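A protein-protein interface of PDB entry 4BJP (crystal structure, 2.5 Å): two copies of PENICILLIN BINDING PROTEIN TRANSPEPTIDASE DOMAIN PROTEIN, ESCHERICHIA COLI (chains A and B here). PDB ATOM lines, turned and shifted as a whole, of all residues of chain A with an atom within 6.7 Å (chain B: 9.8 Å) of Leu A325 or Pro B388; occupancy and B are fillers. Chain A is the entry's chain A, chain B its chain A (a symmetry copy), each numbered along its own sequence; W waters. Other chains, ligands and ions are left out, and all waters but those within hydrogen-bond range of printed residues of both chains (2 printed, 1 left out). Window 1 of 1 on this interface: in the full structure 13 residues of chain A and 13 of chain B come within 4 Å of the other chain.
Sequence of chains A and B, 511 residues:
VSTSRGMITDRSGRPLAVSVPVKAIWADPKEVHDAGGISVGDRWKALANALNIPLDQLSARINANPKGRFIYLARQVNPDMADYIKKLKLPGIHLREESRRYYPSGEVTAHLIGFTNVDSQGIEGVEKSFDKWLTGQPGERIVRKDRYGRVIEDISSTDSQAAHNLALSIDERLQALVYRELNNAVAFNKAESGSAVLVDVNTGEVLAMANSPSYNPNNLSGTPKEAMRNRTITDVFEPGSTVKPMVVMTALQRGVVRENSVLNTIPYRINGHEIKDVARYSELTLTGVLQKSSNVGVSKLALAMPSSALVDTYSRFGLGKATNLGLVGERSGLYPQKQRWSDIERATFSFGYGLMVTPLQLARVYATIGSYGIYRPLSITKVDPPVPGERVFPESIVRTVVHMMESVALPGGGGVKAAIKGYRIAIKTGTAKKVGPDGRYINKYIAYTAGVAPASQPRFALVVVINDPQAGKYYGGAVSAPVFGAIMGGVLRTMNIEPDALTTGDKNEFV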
ATOM      1  N   LEU A 112      -2.650  20.111  13.773  1.00  0.00           N
ATOM      2  CA  LEU A 112      -1.765  19.715  12.688  1.00  0.00           C
ATOM      3  C   LEU A 112      -0.503  18.989  13.179  1.00  0.00           C
ATOM      4  O   LEU A 112      -0.218  17.874  12.741  1.00  0.00           O
ATOM      5  CB  LEU A 112      -1.421  20.902  11.788  1.00  0.00           C
ATOM      6  CG  LEU A 112      -0.434  20.541  10.674  1.00  0.00           C
ATOM      7  CD1 LEU A 112      -1.039  19.581   9.655  1.00  0.00           C
ATOM      8  CD2 LEU A 112       0.095  21.763  10.003  1.00  0.00           C
ATOM      9  N   SER A 129       2.574  11.072  11.899  1.00  0.00           N
ATOM     10  CA  SER A 129       2.475  10.836  10.457  1.00  0.00           C
ATOM     11  C   SER A 129       3.835  10.776   9.789  1.00  0.00           C
ATOM     12  O   SER A 129       4.048   9.976   8.895  1.00  0.00           O
ATOM     13  CB  SER A 129       1.617  11.929   9.817  1.00  0.00           C
ATOM     14  OG  SER A 129       0.262  11.745  10.185  1.00  0.00           O
ATOM     15  N   PHE A 130       4.758  11.617  10.240  1.00  0.00           N
ATOM     16  CA  PHE A 130       6.109  11.620   9.715  1.00  0.00           C
ATOM     17  C   PHE A 130       7.149  11.139  10.741  1.00  0.00           C
ATOM     18  O   PHE A 130       8.311  11.566  10.712  1.00  0.00           O
ATOM     19  CB  PHE A 130       6.437  13.002   9.133  1.00  0.00           C
ATOM     20  CG  PHE A 130       5.501  13.423   8.026  1.00  0.00           C
ATOM     21  CD1 PHE A 130       4.280  14.032   8.311  1.00  0.00           C
ATOM     22  CD2 PHE A 130       5.825  13.198   6.700  1.00  0.00           C
ATOM     23  CE1 PHE A 130       3.408  14.406   7.278  1.00  0.00           C
ATOM     24  CE2 PHE A 130       4.943  13.580   5.670  1.00  0.00           C
ATOM     25  CZ  PHE A 130       3.739  14.183   5.969  1.00  0.00           C
ATOM     26  N   GLY A 204      -0.890  24.084  -4.582  1.00  0.00           N
ATOM     27  CA  GLY A 204      -1.481  23.006  -3.786  1.00  0.00           C
ATOM     28  C   GLY A 204      -1.091  23.046  -2.310  1.00  0.00           C
ATOM     29  O   GLY A 204      -1.573  22.235  -1.510  1.00  0.00           O
ATOM     30  N   VAL A 206      -0.816  23.682   1.573  1.00  0.00           N
ATOM     31  CA  VAL A 206      -1.648  24.093   2.686  1.00  0.00           C
ATOM     32  C   VAL A 206      -0.903  25.176   3.472  1.00  0.00           C
ATOM     33  O   VAL A 206       0.102  24.895   4.120  1.00  0.00           O
ATOM     34  CB  VAL A 206      -2.040  22.893   3.596  1.00  0.00           C
ATOM     35  CG1 VAL A 206      -2.928  23.360   4.738  1.00  0.00           C
ATOM     36  CG2 VAL A 206      -2.770  21.846   2.773  1.00  0.00           C
ATOM     37  N   MET A 209      -3.999  25.622   8.475  1.00  0.00           N
ATOM     38  CA  MET A 209      -4.908  24.521   8.777  1.00  0.00           C
ATOM     39  C   MET A 209      -5.147  24.605  10.279  1.00  0.00           C
ATOM     40  O   MET A 209      -4.242  24.305  11.077  1.00  0.00           O
ATOM     41  CB  MET A 209      -4.263  23.179   8.388  1.00  0.00           C
ATOM     42  CG  MET A 209      -4.954  21.948   8.949  1.00  0.00           C
ATOM     43  SD  MET A 209      -4.361  20.362   8.264  1.00  0.00           S
ATOM     44  CE  MET A 209      -5.286  20.275   6.734  1.00  0.00           C
ATOM     45  N   ILE A 233      -9.559  17.509   8.593  1.00  0.00           N
ATOM     46  CA  ILE A 233      -9.403  16.252   7.837  1.00  0.00           C
ATOM     47  C   ILE A 233     -10.265  15.080   8.361  1.00  0.00           C
ATOM     48  O   ILE A 233     -10.489  14.127   7.625  1.00  0.00           O
ATOM     49  CB  ILE A 233      -7.921  15.820   7.733  1.00  0.00           C
ATOM     50  CG1 ILE A 233      -7.390  15.356   9.106  1.00  0.00           C
ATOM     51  CG2 ILE A 233      -7.101  16.924   7.117  1.00  0.00           C
ATOM     52  CD1 ILE A 233      -5.991  14.752   9.082  1.00  0.00           C
ATOM     53  N   ALA A 322      -9.419  10.951  -2.087  1.00  0.00           N
ATOM     54  CA  ALA A 322      -8.507  11.130  -0.973  1.00  0.00           C
ATOM     55  C   ALA A 322      -7.698  12.422  -1.146  1.00  0.00           C
ATOM     56  O   ALA A 322      -7.368  12.822  -2.292  1.00  0.00           O
ATOM     57  CB  ALA A 322      -7.601   9.915  -0.826  1.00  0.00           C
ATOM     58  N   THR A 323      -7.377  13.065  -0.016  1.00  0.00           N
ATOM     59  CA  THR A 323      -6.590  14.318  -0.057  1.00  0.00           C
ATOM     60  C   THR A 323      -5.092  14.095   0.029  1.00  0.00           C
ATOM     61  O   THR A 323      -4.314  14.996  -0.263  1.00  0.00           O
ATOM     62  CB  THR A 323      -7.036  15.339   1.016  1.00  0.00           C
ATOM     63  OG1 THR A 323      -7.108  14.711   2.298  1.00  0.00           O
ATOM     64  CG2 THR A 323      -8.419  15.927   0.651  1.00  0.00           C
ATOM     65  N   ASN A 324      -4.682  12.903   0.450  1.00  0.00           N
ATOM     66  CA  ASN A 324      -3.271  12.482   0.367  1.00  0.00           C
ATOM     67  C   ASN A 324      -2.204  13.365   1.012  1.00  0.00           C
ATOM     68  O   ASN A 324      -1.085  13.408   0.526  1.00  0.00           O
ATOM     69  CB  ASN A 324      -2.871  12.215  -1.093  1.00  0.00           C
ATOM     70  CG  ASN A 324      -3.819  11.259  -1.780  1.00  0.00           C
ATOM     71  OD1 ASN A 324      -4.254  11.500  -2.900  1.00  0.00           O
ATOM     72  ND2 ASN A 324      -4.154  10.173  -1.104  1.00  0.00           N
ATOM     73  N   LEU A 325      -2.516  14.029   2.117  1.00  0.00           N
ATOM     74  CA  LEU A 325      -1.479  14.750   2.870  1.00  0.00           C
ATOM     75  C   LEU A 325      -0.488  13.830   3.596  1.00  0.00           C
ATOM     76  O   LEU A 325       0.665  14.212   3.782  1.00  0.00           O
ATOM     77  CB  LEU A 325      -2.103  15.728   3.888  1.00  0.00           C
ATOM     78  CG  LEU A 325      -2.813  16.955   3.324  1.00  0.00           C
ATOM     79  CD1 LEU A 325      -3.164  17.921   4.469  1.00  0.00           C
ATOM     80  CD2 LEU A 325      -1.978  17.644   2.244  1.00  0.00           C
ATOM     81  N   GLY A 326      -0.944  12.635   3.989  1.00  0.00           N
ATOM     82  CA  GLY A 326      -0.128  11.676   4.761  1.00  0.00           C
ATOM     83  C   GLY A 326      -0.406  11.714   6.261  1.00  0.00           C
ATOM     84  O   GLY A 326       0.309  11.113   7.083  1.00  0.00           O
ATOM     85  N   LEU A 327      -1.459  12.430   6.611  1.00  0.00           N
ATOM     86  CA  LEU A 327      -1.806  12.664   7.980  1.00  0.00           C
ATOM     87  C   LEU A 327      -2.702  11.561   8.506  1.00  0.00           C
ATOM     88  O   LEU A 327      -3.647  11.137   7.833  1.00  0.00           O
ATOM     89  CB  LEU A 327      -2.495  14.023   8.091  1.00  0.00           C
ATOM     90  CG  LEU A 327      -1.666  15.251   7.718  1.00  0.00           C
ATOM     91  CD1 LEU A 327      -2.500  16.502   7.921  1.00  0.00           C
ATOM     92  CD2 LEU A 327      -0.349  15.334   8.530  1.00  0.00           C
ATOM     93  N   GLU A 330      -6.891  11.116   8.292  1.00  0.00           N
ATOM     94  CA  GLU A 330      -7.335  11.782   7.054  1.00  0.00           C
ATOM     95  C   GLU A 330      -8.464  11.020   6.352  1.00  0.00           C
ATOM     96  O   GLU A 330      -8.341   9.838   6.032  1.00  0.00           O
ATOM     97  CB  GLU A 330      -6.156  11.960   6.105  1.00  0.00           C
ATOM     98  CG  GLU A 330      -6.283  13.105   5.130  1.00  0.00           C
ATOM     99  CD  GLU A 330      -4.952  13.451   4.465  1.00  0.00           C
ATOM    100  OE1 GLU A 330      -3.889  13.150   5.062  1.00  0.00           O
ATOM    101  OE2 GLU A 330      -4.973  14.015   3.346  1.00  0.00           O
ATOM    102  N   LEU A 360     -10.925  20.120   4.212  1.00  0.00           N
ATOM    103  CA  LEU A 360      -9.779  20.097   3.307  1.00  0.00           C
ATOM    104  C   LEU A 360     -10.160  19.806   1.842  1.00  0.00           C
ATOM    105  O   LEU A 360      -9.609  20.445   0.940  1.00  0.00           O
ATOM    106  CB  LEU A 360      -8.711  19.112   3.780  1.00  0.00           C
ATOM    107  CG  LEU A 360      -7.398  19.027   2.999  1.00  0.00           C
ATOM    108  CD1 LEU A 360      -6.586  20.336   3.021  1.00  0.00           C
ATOM    109  CD2 LEU A 360      -6.580  17.886   3.563  1.00  0.00           C
ATOM    110  N   PRO A 377      -2.497  18.381  -6.772  1.00  0.00           N
ATOM    111  CA  PRO A 377      -2.546  17.675  -5.493  1.00  0.00           C
ATOM    112  C   PRO A 377      -2.123  18.604  -4.347  1.00  0.00           C
ATOM    113  O   PRO A 377      -1.304  19.476  -4.566  1.00  0.00           O
ATOM    114  CB  PRO A 377      -1.528  16.552  -5.674  1.00  0.00           C
ATOM    115  CG  PRO A 377      -0.543  17.090  -6.711  1.00  0.00           C
ATOM    116  CD  PRO A 377      -1.336  18.002  -7.606  1.00  0.00           C
ATOM    117  N   LEU A 378      -2.697  18.413  -3.157  1.00  0.00           N
ATOM    118  CA  LEU A 378      -2.353  19.175  -1.952  1.00  0.00           C
ATOM    119  C   LEU A 378      -1.058  18.697  -1.299  1.00  0.00           C
ATOM    120  O   LEU A 378      -0.621  17.591  -1.548  1.00  0.00           O
ATOM    121  CB  LEU A 378      -3.482  19.059  -0.932  1.00  0.00           C
ATOM    122  CG  LEU A 378      -4.873  19.522  -1.344  1.00  0.00           C
ATOM    123  CD1 LEU A 378      -5.902  18.599  -0.689  1.00  0.00           C
ATOM    124  CD2 LEU A 378      -5.107  20.991  -0.998  1.00  0.00           C
ATOM    125  N   SER A 379      -0.479  19.517  -0.425  1.00  0.00           N
ATOM    126  CA  SER A 379       0.794  19.205   0.240  1.00  0.00           C
ATOM    127  C   SER A 379       0.831  19.911   1.601  1.00  0.00           C
ATOM    128  O   SER A 379       0.570  21.124   1.651  1.00  0.00           O
ATOM    129  CB  SER A 379       1.937  19.692  -0.674  1.00  0.00           C
ATOM    130  OG  SER A 379       3.218  19.173  -0.323  1.00  0.00           O
ATOM    131  N   ILE A 380       1.098  19.191   2.705  1.00  0.00           N
ATOM    132  CA  ILE A 380       1.492  19.897   3.947  1.00  0.00           C
ATOM    133  C   ILE A 380       2.987  20.130   4.066  1.00  0.00           C
ATOM    134  O   ILE A 380       3.444  20.666   5.071  1.00  0.00           O
ATOM    135  CB  ILE A 380       1.029  19.268   5.326  1.00  0.00           C
ATOM    136  CG1 ILE A 380       0.830  17.770   5.218  1.00  0.00           C
ATOM    137  CG2 ILE A 380      -0.167  20.068   5.962  1.00  0.00           C
ATOM    138  CD1 ILE A 380       2.103  17.012   5.296  1.00  0.00           C
ATOM    139  N   THR A 381       3.756  19.712   3.074  1.00  0.00           N
ATOM    140  CA  THR A 381       5.170  20.053   3.095  1.00  0.00           C
ATOM    141  C   THR A 381       5.435  21.100   2.024  1.00  0.00           C
ATOM    142  O   THR A 381       4.687  21.213   1.049  1.00  0.00           O
ATOM    143  CB  THR A 381       6.103  18.827   2.958  1.00  0.00           C
ATOM    144  OG1 THR A 381       5.908  18.206   1.679  1.00  0.00           O
ATOM    145  CG2 THR A 381       5.840  17.806   4.086  1.00  0.00           C
ATOM    146  N   VAL B 201      11.457   5.719  -7.236  1.00  0.00           N
ATOM    147  CA  VAL B 201      10.296   5.006  -6.693  1.00  0.00           C
ATOM    148  C   VAL B 201       9.672   5.738  -5.511  1.00  0.00           C
ATOM    149  O   VAL B 201       8.478   5.610  -5.252  1.00  0.00           O
ATOM    150  CB  VAL B 201      10.672   3.541  -6.267  1.00  0.00           C
ATOM    151  CG1 VAL B 201       9.690   2.987  -5.245  1.00  0.00           C
ATOM    152  CG2 VAL B 201      10.752   2.633  -7.493  1.00  0.00           C
ATOM    153  N   ASN B 202      10.480   6.510  -4.800  1.00  0.00           N
ATOM    154  CA  ASN B 202      10.020   7.120  -3.556  1.00  0.00           C
ATOM    155  C   ASN B 202       9.495   8.535  -3.720  1.00  0.00           C
ATOM    156  O   ASN B 202       8.798   9.041  -2.834  1.00  0.00           O
ATOM    157  CB  ASN B 202      11.123   7.057  -2.492  1.00  0.00           C
ATOM    158  CG  ASN B 202      11.370   5.628  -1.992  1.00  0.00           C
ATOM    159  OD1 ASN B 202      12.482   5.115  -2.088  1.00  0.00           O
ATOM    160  ND2 ASN B 202      10.319   4.976  -1.472  1.00  0.00           N
ATOM    161  N   THR B 203       9.783   9.160  -4.861  1.00  0.00           N
ATOM    162  CA  THR B 203       9.445  10.571  -5.035  1.00  0.00           C
ATOM    163  C   THR B 203       8.596  10.928  -6.264  1.00  0.00           C
ATOM    164  O   THR B 203       8.039  12.020  -6.327  1.00  0.00           O
ATOM    165  CB  THR B 203      10.718  11.488  -5.025  1.00  0.00           C
ATOM    166  OG1 THR B 203      11.473  11.268  -6.205  1.00  0.00           O
ATOM    167  CG2 THR B 203      11.609  11.204  -3.833  1.00  0.00           C
ATOM    168  N   GLY B 204       8.500  10.031  -7.244  1.00  0.00           N
ATOM    169  CA  GLY B 204       7.858  10.375  -8.514  1.00  0.00           C
ATOM    170  C   GLY B 204       8.777  11.113  -9.487  1.00  0.00           C
ATOM    171  O   GLY B 204       8.384  11.404 -10.624  1.00  0.00           O
ATOM    172  N   SER B 371       6.842   0.727  -5.224  1.00  0.00           N
ATOM    173  CA  SER B 371       6.528   1.274  -3.908  1.00  0.00           C
ATOM    174  C   SER B 371       5.600   0.321  -3.185  1.00  0.00           C
ATOM    175  O   SER B 371       5.144   0.606  -2.078  1.00  0.00           O
ATOM    176  CB  SER B 371       5.865   2.623  -4.046  1.00  0.00           C
ATOM    177  OG  SER B 371       4.652   2.509  -4.757  1.00  0.00           O
ATOM    178  N   GLY B 373       2.575  -0.490  -4.198  1.00  0.00           N
ATOM    179  CA  GLY B 373       1.179  -0.094  -4.316  1.00  0.00           C
ATOM    180  C   GLY B 373       0.887   1.337  -3.970  1.00  0.00           C
ATOM    181  O   GLY B 373      -0.264   1.707  -3.820  1.00  0.00           O
ATOM    182  N   ILE B 374       1.925   2.154  -3.832  1.00  0.00           N
ATOM    183  CA  ILE B 374       1.731   3.571  -3.568  1.00  0.00           C
ATOM    184  C   ILE B 374       1.873   4.366  -4.870  1.00  0.00           C
ATOM    185  O   ILE B 374       2.922   4.379  -5.484  1.00  0.00           O
ATOM    186  CB  ILE B 374       2.711   4.081  -2.469  1.00  0.00           C
ATOM    187  CG1 ILE B 374       2.343   3.458  -1.114  1.00  0.00           C
ATOM    188  CG2 ILE B 374       2.699   5.621  -2.379  1.00  0.00           C
ATOM    189  CD1 ILE B 374       3.464   3.492  -0.080  1.00  0.00           C
ATOM    190  N   TYR B 375       0.789   5.014  -5.279  1.00  0.00           N
ATOM    191  CA  TYR B 375       0.762   5.878  -6.456  1.00  0.00           C
ATOM    192  C   TYR B 375       1.209   7.292  -6.081  1.00  0.00           C
ATOM    193  O   TYR B 375       0.698   7.887  -5.118  1.00  0.00           O
ATOM    194  CB  TYR B 375      -0.661   5.924  -6.991  1.00  0.00           C
ATOM    195  CG  TYR B 375      -0.844   6.594  -8.335  1.00  0.00           C
ATOM    196  CD1 TYR B 375      -0.441   5.959  -9.506  1.00  0.00           C
ATOM    197  CD2 TYR B 375      -1.470   7.848  -8.438  1.00  0.00           C
ATOM    198  CE1 TYR B 375      -0.616   6.553 -10.742  1.00  0.00           C
ATOM    199  CE2 TYR B 375      -1.666   8.460  -9.685  1.00  0.00           C
ATOM    200  CZ  TYR B 375      -1.232   7.796 -10.838  1.00  0.00           C
ATOM    201  OH  TYR B 375      -1.413   8.341 -12.092  1.00  0.00           O
ATOM    202  N   ARG B 376       2.166   7.809  -6.840  1.00  0.00           N
ATOM    203  CA  ARG B 376       2.724   9.144  -6.659  1.00  0.00           C
ATOM    204  C   ARG B 376       2.716   9.823  -8.015  1.00  0.00           C
ATOM    205  O   ARG B 376       3.048   9.199  -9.023  1.00  0.00           O
ATOM    206  CB  ARG B 376       4.166   9.097  -6.111  1.00  0.00           C
ATOM    207  CG  ARG B 376       4.264   8.396  -4.747  1.00  0.00           C
ATOM    208  CD  ARG B 376       5.564   8.682  -3.978  1.00  0.00           C
ATOM    209  NE  ARG B 376       6.200   7.420  -3.656  1.00  0.00           N
ATOM    210  CZ  ARG B 376       6.216   6.828  -2.470  1.00  0.00           C
ATOM    211  NH1 ARG B 376       5.676   7.399  -1.424  1.00  0.00           N
ATOM    212  NH2 ARG B 376       6.821   5.653  -2.342  1.00  0.00           N
ATOM    213  N   PRO B 377       2.328  11.102  -8.050  1.00  0.00           N
ATOM    214  CA  PRO B 377       2.408  11.826  -9.316  1.00  0.00           C
ATOM    215  C   PRO B 377       3.872  12.020  -9.736  1.00  0.00           C
ATOM    216  O   PRO B 377       4.721  12.142  -8.875  1.00  0.00           O
ATOM    217  CB  PRO B 377       1.763  13.171  -8.993  1.00  0.00           C
ATOM    218  CG  PRO B 377       1.983  13.351  -7.491  1.00  0.00           C
ATOM    219  CD  PRO B 377       1.985  11.967  -6.901  1.00  0.00           C
ATOM    220  N   VAL B 383      12.062  17.613  -6.478  1.00  0.00           N
ATOM    221  CA  VAL B 383      11.042  17.533  -5.433  1.00  0.00           C
ATOM    222  C   VAL B 383      11.690  17.051  -4.158  1.00  0.00           C
ATOM    223  O   VAL B 383      12.454  16.090  -4.192  1.00  0.00           O
ATOM    224  CB  VAL B 383       9.913  16.546  -5.832  1.00  0.00           C
ATOM    225  CG1 VAL B 383       9.286  15.897  -4.601  1.00  0.00           C
ATOM    226  CG2 VAL B 383       8.853  17.258  -6.664  1.00  0.00           C
ATOM    227  N   ASP B 384      11.395  17.693  -3.031  1.00  0.00           N
ATOM    228  CA  ASP B 384      11.906  17.191  -1.746  1.00  0.00           C
ATOM    229  C   ASP B 384      10.995  16.121  -1.108  1.00  0.00           C
ATOM    230  O   ASP B 384       9.768  16.298  -1.044  1.00  0.00           O
ATOM    231  CB  ASP B 384      12.157  18.343  -0.774  1.00  0.00           C
ATOM    232  CG  ASP B 384      13.083  19.403  -1.354  1.00  0.00           C
ATOM    233  OD1 ASP B 384      14.228  19.050  -1.740  1.00  0.00           O
ATOM    234  OD2 ASP B 384      12.660  20.587  -1.427  1.00  0.00           O
ATOM    235  N   PRO B 385      11.589  15.002  -0.643  1.00  0.00           N
ATOM    236  CA  PRO B 385      10.856  14.030   0.169  1.00  0.00           C
ATOM    237  C   PRO B 385      10.434  14.644   1.518  1.00  0.00           C
ATOM    238  O   PRO B 385      11.017  15.643   1.954  1.00  0.00           O
ATOM    239  CB  PRO B 385      11.892  12.911   0.413  1.00  0.00           C
ATOM    240  CG  PRO B 385      13.009  13.171  -0.500  1.00  0.00           C
ATOM    241  CD  PRO B 385      13.010  14.645  -0.764  1.00  0.00           C
ATOM    242  N   PRO B 386       9.438  14.052   2.186  1.00  0.00           N
ATOM    243  CA  PRO B 386       8.714  12.856   1.762  1.00  0.00           C
ATOM    244  C   PRO B 386       7.546  13.166   0.808  1.00  0.00           C
ATOM    245  O   PRO B 386       7.007  14.274   0.836  1.00  0.00           O
ATOM    246  CB  PRO B 386       8.204  12.276   3.084  1.00  0.00           C
ATOM    247  CG  PRO B 386       8.302  13.400   4.099  1.00  0.00           C
ATOM    248  CD  PRO B 386       8.919  14.589   3.453  1.00  0.00           C
ATOM    249  N   VAL B 387       7.192  12.201  -0.044  1.00  0.00           N
ATOM    250  CA  VAL B 387       6.010  12.297  -0.900  1.00  0.00           C
ATOM    251  C   VAL B 387       5.104  11.139  -0.521  1.00  0.00           C
ATOM    252  O   VAL B 387       5.378  10.013  -0.892  1.00  0.00           O
ATOM    253  CB  VAL B 387       6.362  12.210  -2.387  1.00  0.00           C
ATOM    254  CG1 VAL B 387       5.091  12.139  -3.254  1.00  0.00           C
ATOM    255  CG2 VAL B 387       7.224  13.397  -2.797  1.00  0.00           C
ATOM    256  N   PRO B 388       4.043  11.415   0.265  1.00  0.00           N
ATOM    257  CA  PRO B 388       3.179  10.349   0.758  1.00  0.00           C
ATOM    258  C   PRO B 388       2.532   9.526  -0.361  1.00  0.00           C
ATOM    259  O   PRO B 388       2.488   8.288  -0.264  1.00  0.00           O
ATOM    260  CB  PRO B 388       2.120  11.105   1.564  1.00  0.00           C
ATOM    261  CG  PRO B 388       2.811  12.347   2.016  1.00  0.00           C
ATOM    262  CD  PRO B 388       3.732  12.716   0.893  1.00  0.00           C
ATOM    263  N   GLY B 389       2.034  10.201  -1.401  1.00  0.00           N
ATOM    264  CA  GLY B 389       1.253   9.540  -2.466  1.00  0.00           C
ATOM    265  C   GLY B 389      -0.034   8.876  -1.965  1.00  0.00           C
ATOM    266  O   GLY B 389      -0.533   9.200  -0.875  1.00  0.00           O
ATOM    267  N   GLU B 390      -0.572   7.935  -2.746  1.00  0.00           N
ATOM    268  CA  GLU B 390      -1.889   7.325  -2.443  1.00  0.00           C
ATOM    269  C   GLU B 390      -1.815   5.829  -2.644  1.00  0.00           C
ATOM    270  O   GLU B 390      -1.434   5.363  -3.710  1.00  0.00           O
ATOM    271  CB  GLU B 390      -3.023   7.918  -3.316  1.00  0.00           C
ATOM    272  CG  GLU B 390      -4.412   7.593  -2.765  1.00  0.00           C
ATOM    273  CD  GLU B 390      -5.602   8.096  -3.597  1.00  0.00           C
ATOM    274  OE1 GLU B 390      -5.447   8.998  -4.446  1.00  0.00           O
ATOM    275  OE2 GLU B 390      -6.722   7.577  -3.383  1.00  0.00           O
ATOM    276  N   ARG B 391      -2.175   5.070  -1.626  1.00  0.00           N
ATOM    277  CA  ARG B 391      -2.151   3.642  -1.777  1.00  0.00           C
ATOM    278  C   ARG B 391      -3.324   3.190  -2.661  1.00  0.00           C
ATOM    279  O   ARG B 391      -4.485   3.515  -2.377  1.00  0.00           O
ATOM    280  CB  ARG B 391      -2.107   2.961  -0.421  1.00  0.00           C
ATOM    281  CG  ARG B 391      -2.857   1.643  -0.308  1.00  0.00           C
ATOM    282  CD  ARG B 391      -2.213   0.800   0.784  1.00  0.00           C
ATOM    283  NE  ARG B 391      -1.187   0.047   0.107  1.00  0.00           N
ATOM    284  CZ  ARG B 391       0.115   0.115   0.312  1.00  0.00           C
ATOM    285  NH1 ARG B 391       0.642   0.865   1.263  1.00  0.00           N
ATOM    286  NH2 ARG B 391       0.874  -0.641  -0.450  1.00  0.00           N
ATOM    287  N   VAL B 392      -2.998   2.491  -3.748  1.00  0.00           N
ATOM    288  CA  VAL B 392      -3.999   2.053  -4.705  1.00  0.00           C
ATOM    289  C   VAL B 392      -4.118   0.522  -4.748  1.00  0.00           C
ATOM    290  O   VAL B 392      -5.034  -0.008  -5.366  1.00  0.00           O
ATOM    291  CB  VAL B 392      -3.746   2.608  -6.141  1.00  0.00           C
ATOM    292  CG1 VAL B 392      -3.868   4.140  -6.177  1.00  0.00           C
ATOM    293  CG2 VAL B 392      -2.377   2.161  -6.666  1.00  0.00           C
HETATM  294  O   HOH W   1       4.837  15.842   1.514  1.00  0.00           O
HETATM  295  O   HOH W   2      -9.089   8.757  -3.799  1.00  0.00           O
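Gly A326 touches just one residue of chain B: Pro B388 (3.9 Å).
No residue of chain B comes within 4 Å of Leu A378.
Printed residues of chain B within 4 Å of Asn A324: Gly B389 and Glu B390.
Of the printed residues of chain A, Gly B389 touches Asn A324.
Of the printed residues of chain B, Ala A322 touches Glu B390.
Of the printed residues of chain A, Glu B390 touches Ala A322 and Asn A324.
Water W1 bridges the side-chain hydroxyl (OG1) of Thr A381 (2.6 Å) and the backbone carbonyl oxygen (O) of Pro B386 (2.8 Å).
Water W2 bridges OE2 of Glu B390 (2.7 Å) and N of Ala A322 (2.8 Å).
2 positions are printed for both chains.
Of the 6 pairs that touch across the chains among the printed residues, none has its exchanged pair printed and touching as well.
O of Gly A326 lies close to OG of Ser A129, 3.2 Å away.
The backbone carbonyl oxygen (O) of Ala A322 lies close to the side-chain amide oxygen (OD1) of Asn A324, at 3.4 Å.
OE2 of Glu A330 lies within hydrogen-bond range of N of Asn A324, 3.1 Å away.
The backbone NH (N) of Leu A325 is in hydrogen-bond range of the side-chain carboxylate (OE2) of Glu A330, at 2.7 Å.
The backbone NH (N) of Gly A326 is in hydrogen-bond range of the side-chain carboxylate (OE1) of Glu A330 (3.2 Å).
The backbone NH (N) of Glu B390 is in hydrogen-bond range of the backbone carbonyl oxygen (O) of Tyr B375.
Printed residues of chain A that touch a printed residue of chain B: Phe A130, Ala A322, Asn A324, Leu A325 and Gly A326.
Printed residues of chain B that touch a printed residue of chain A: Pro B386, Pro B388, Gly B389 and Glu B390.
Hydrophobic or aromatic side chains of chain B within 4 Å of the printed part of chain A: Pro B386 and Pro B388.
Along chain B the printed residues that touch a printed residue of chain A span positions 386 to 390.
Among the printed residues, no Asp or Glu carboxylate lies within 4 Å of a Lys or Arg side-chain nitrogen of the other chain.
Phe A130 touches Pro B386.
CB of Ala A322 touches OE2 of Glu B390, 3.6 Å away.
Asn A324 touches Gly B389.
Leu A325 touches Pro B388 (O to CG, 3.3 Å).
Pro B388 touches Gly A326 (CB to CA, 3.9 Å).
OD1 of Asn A324 lies close to OE1 of Glu B390 (3.2 Å).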
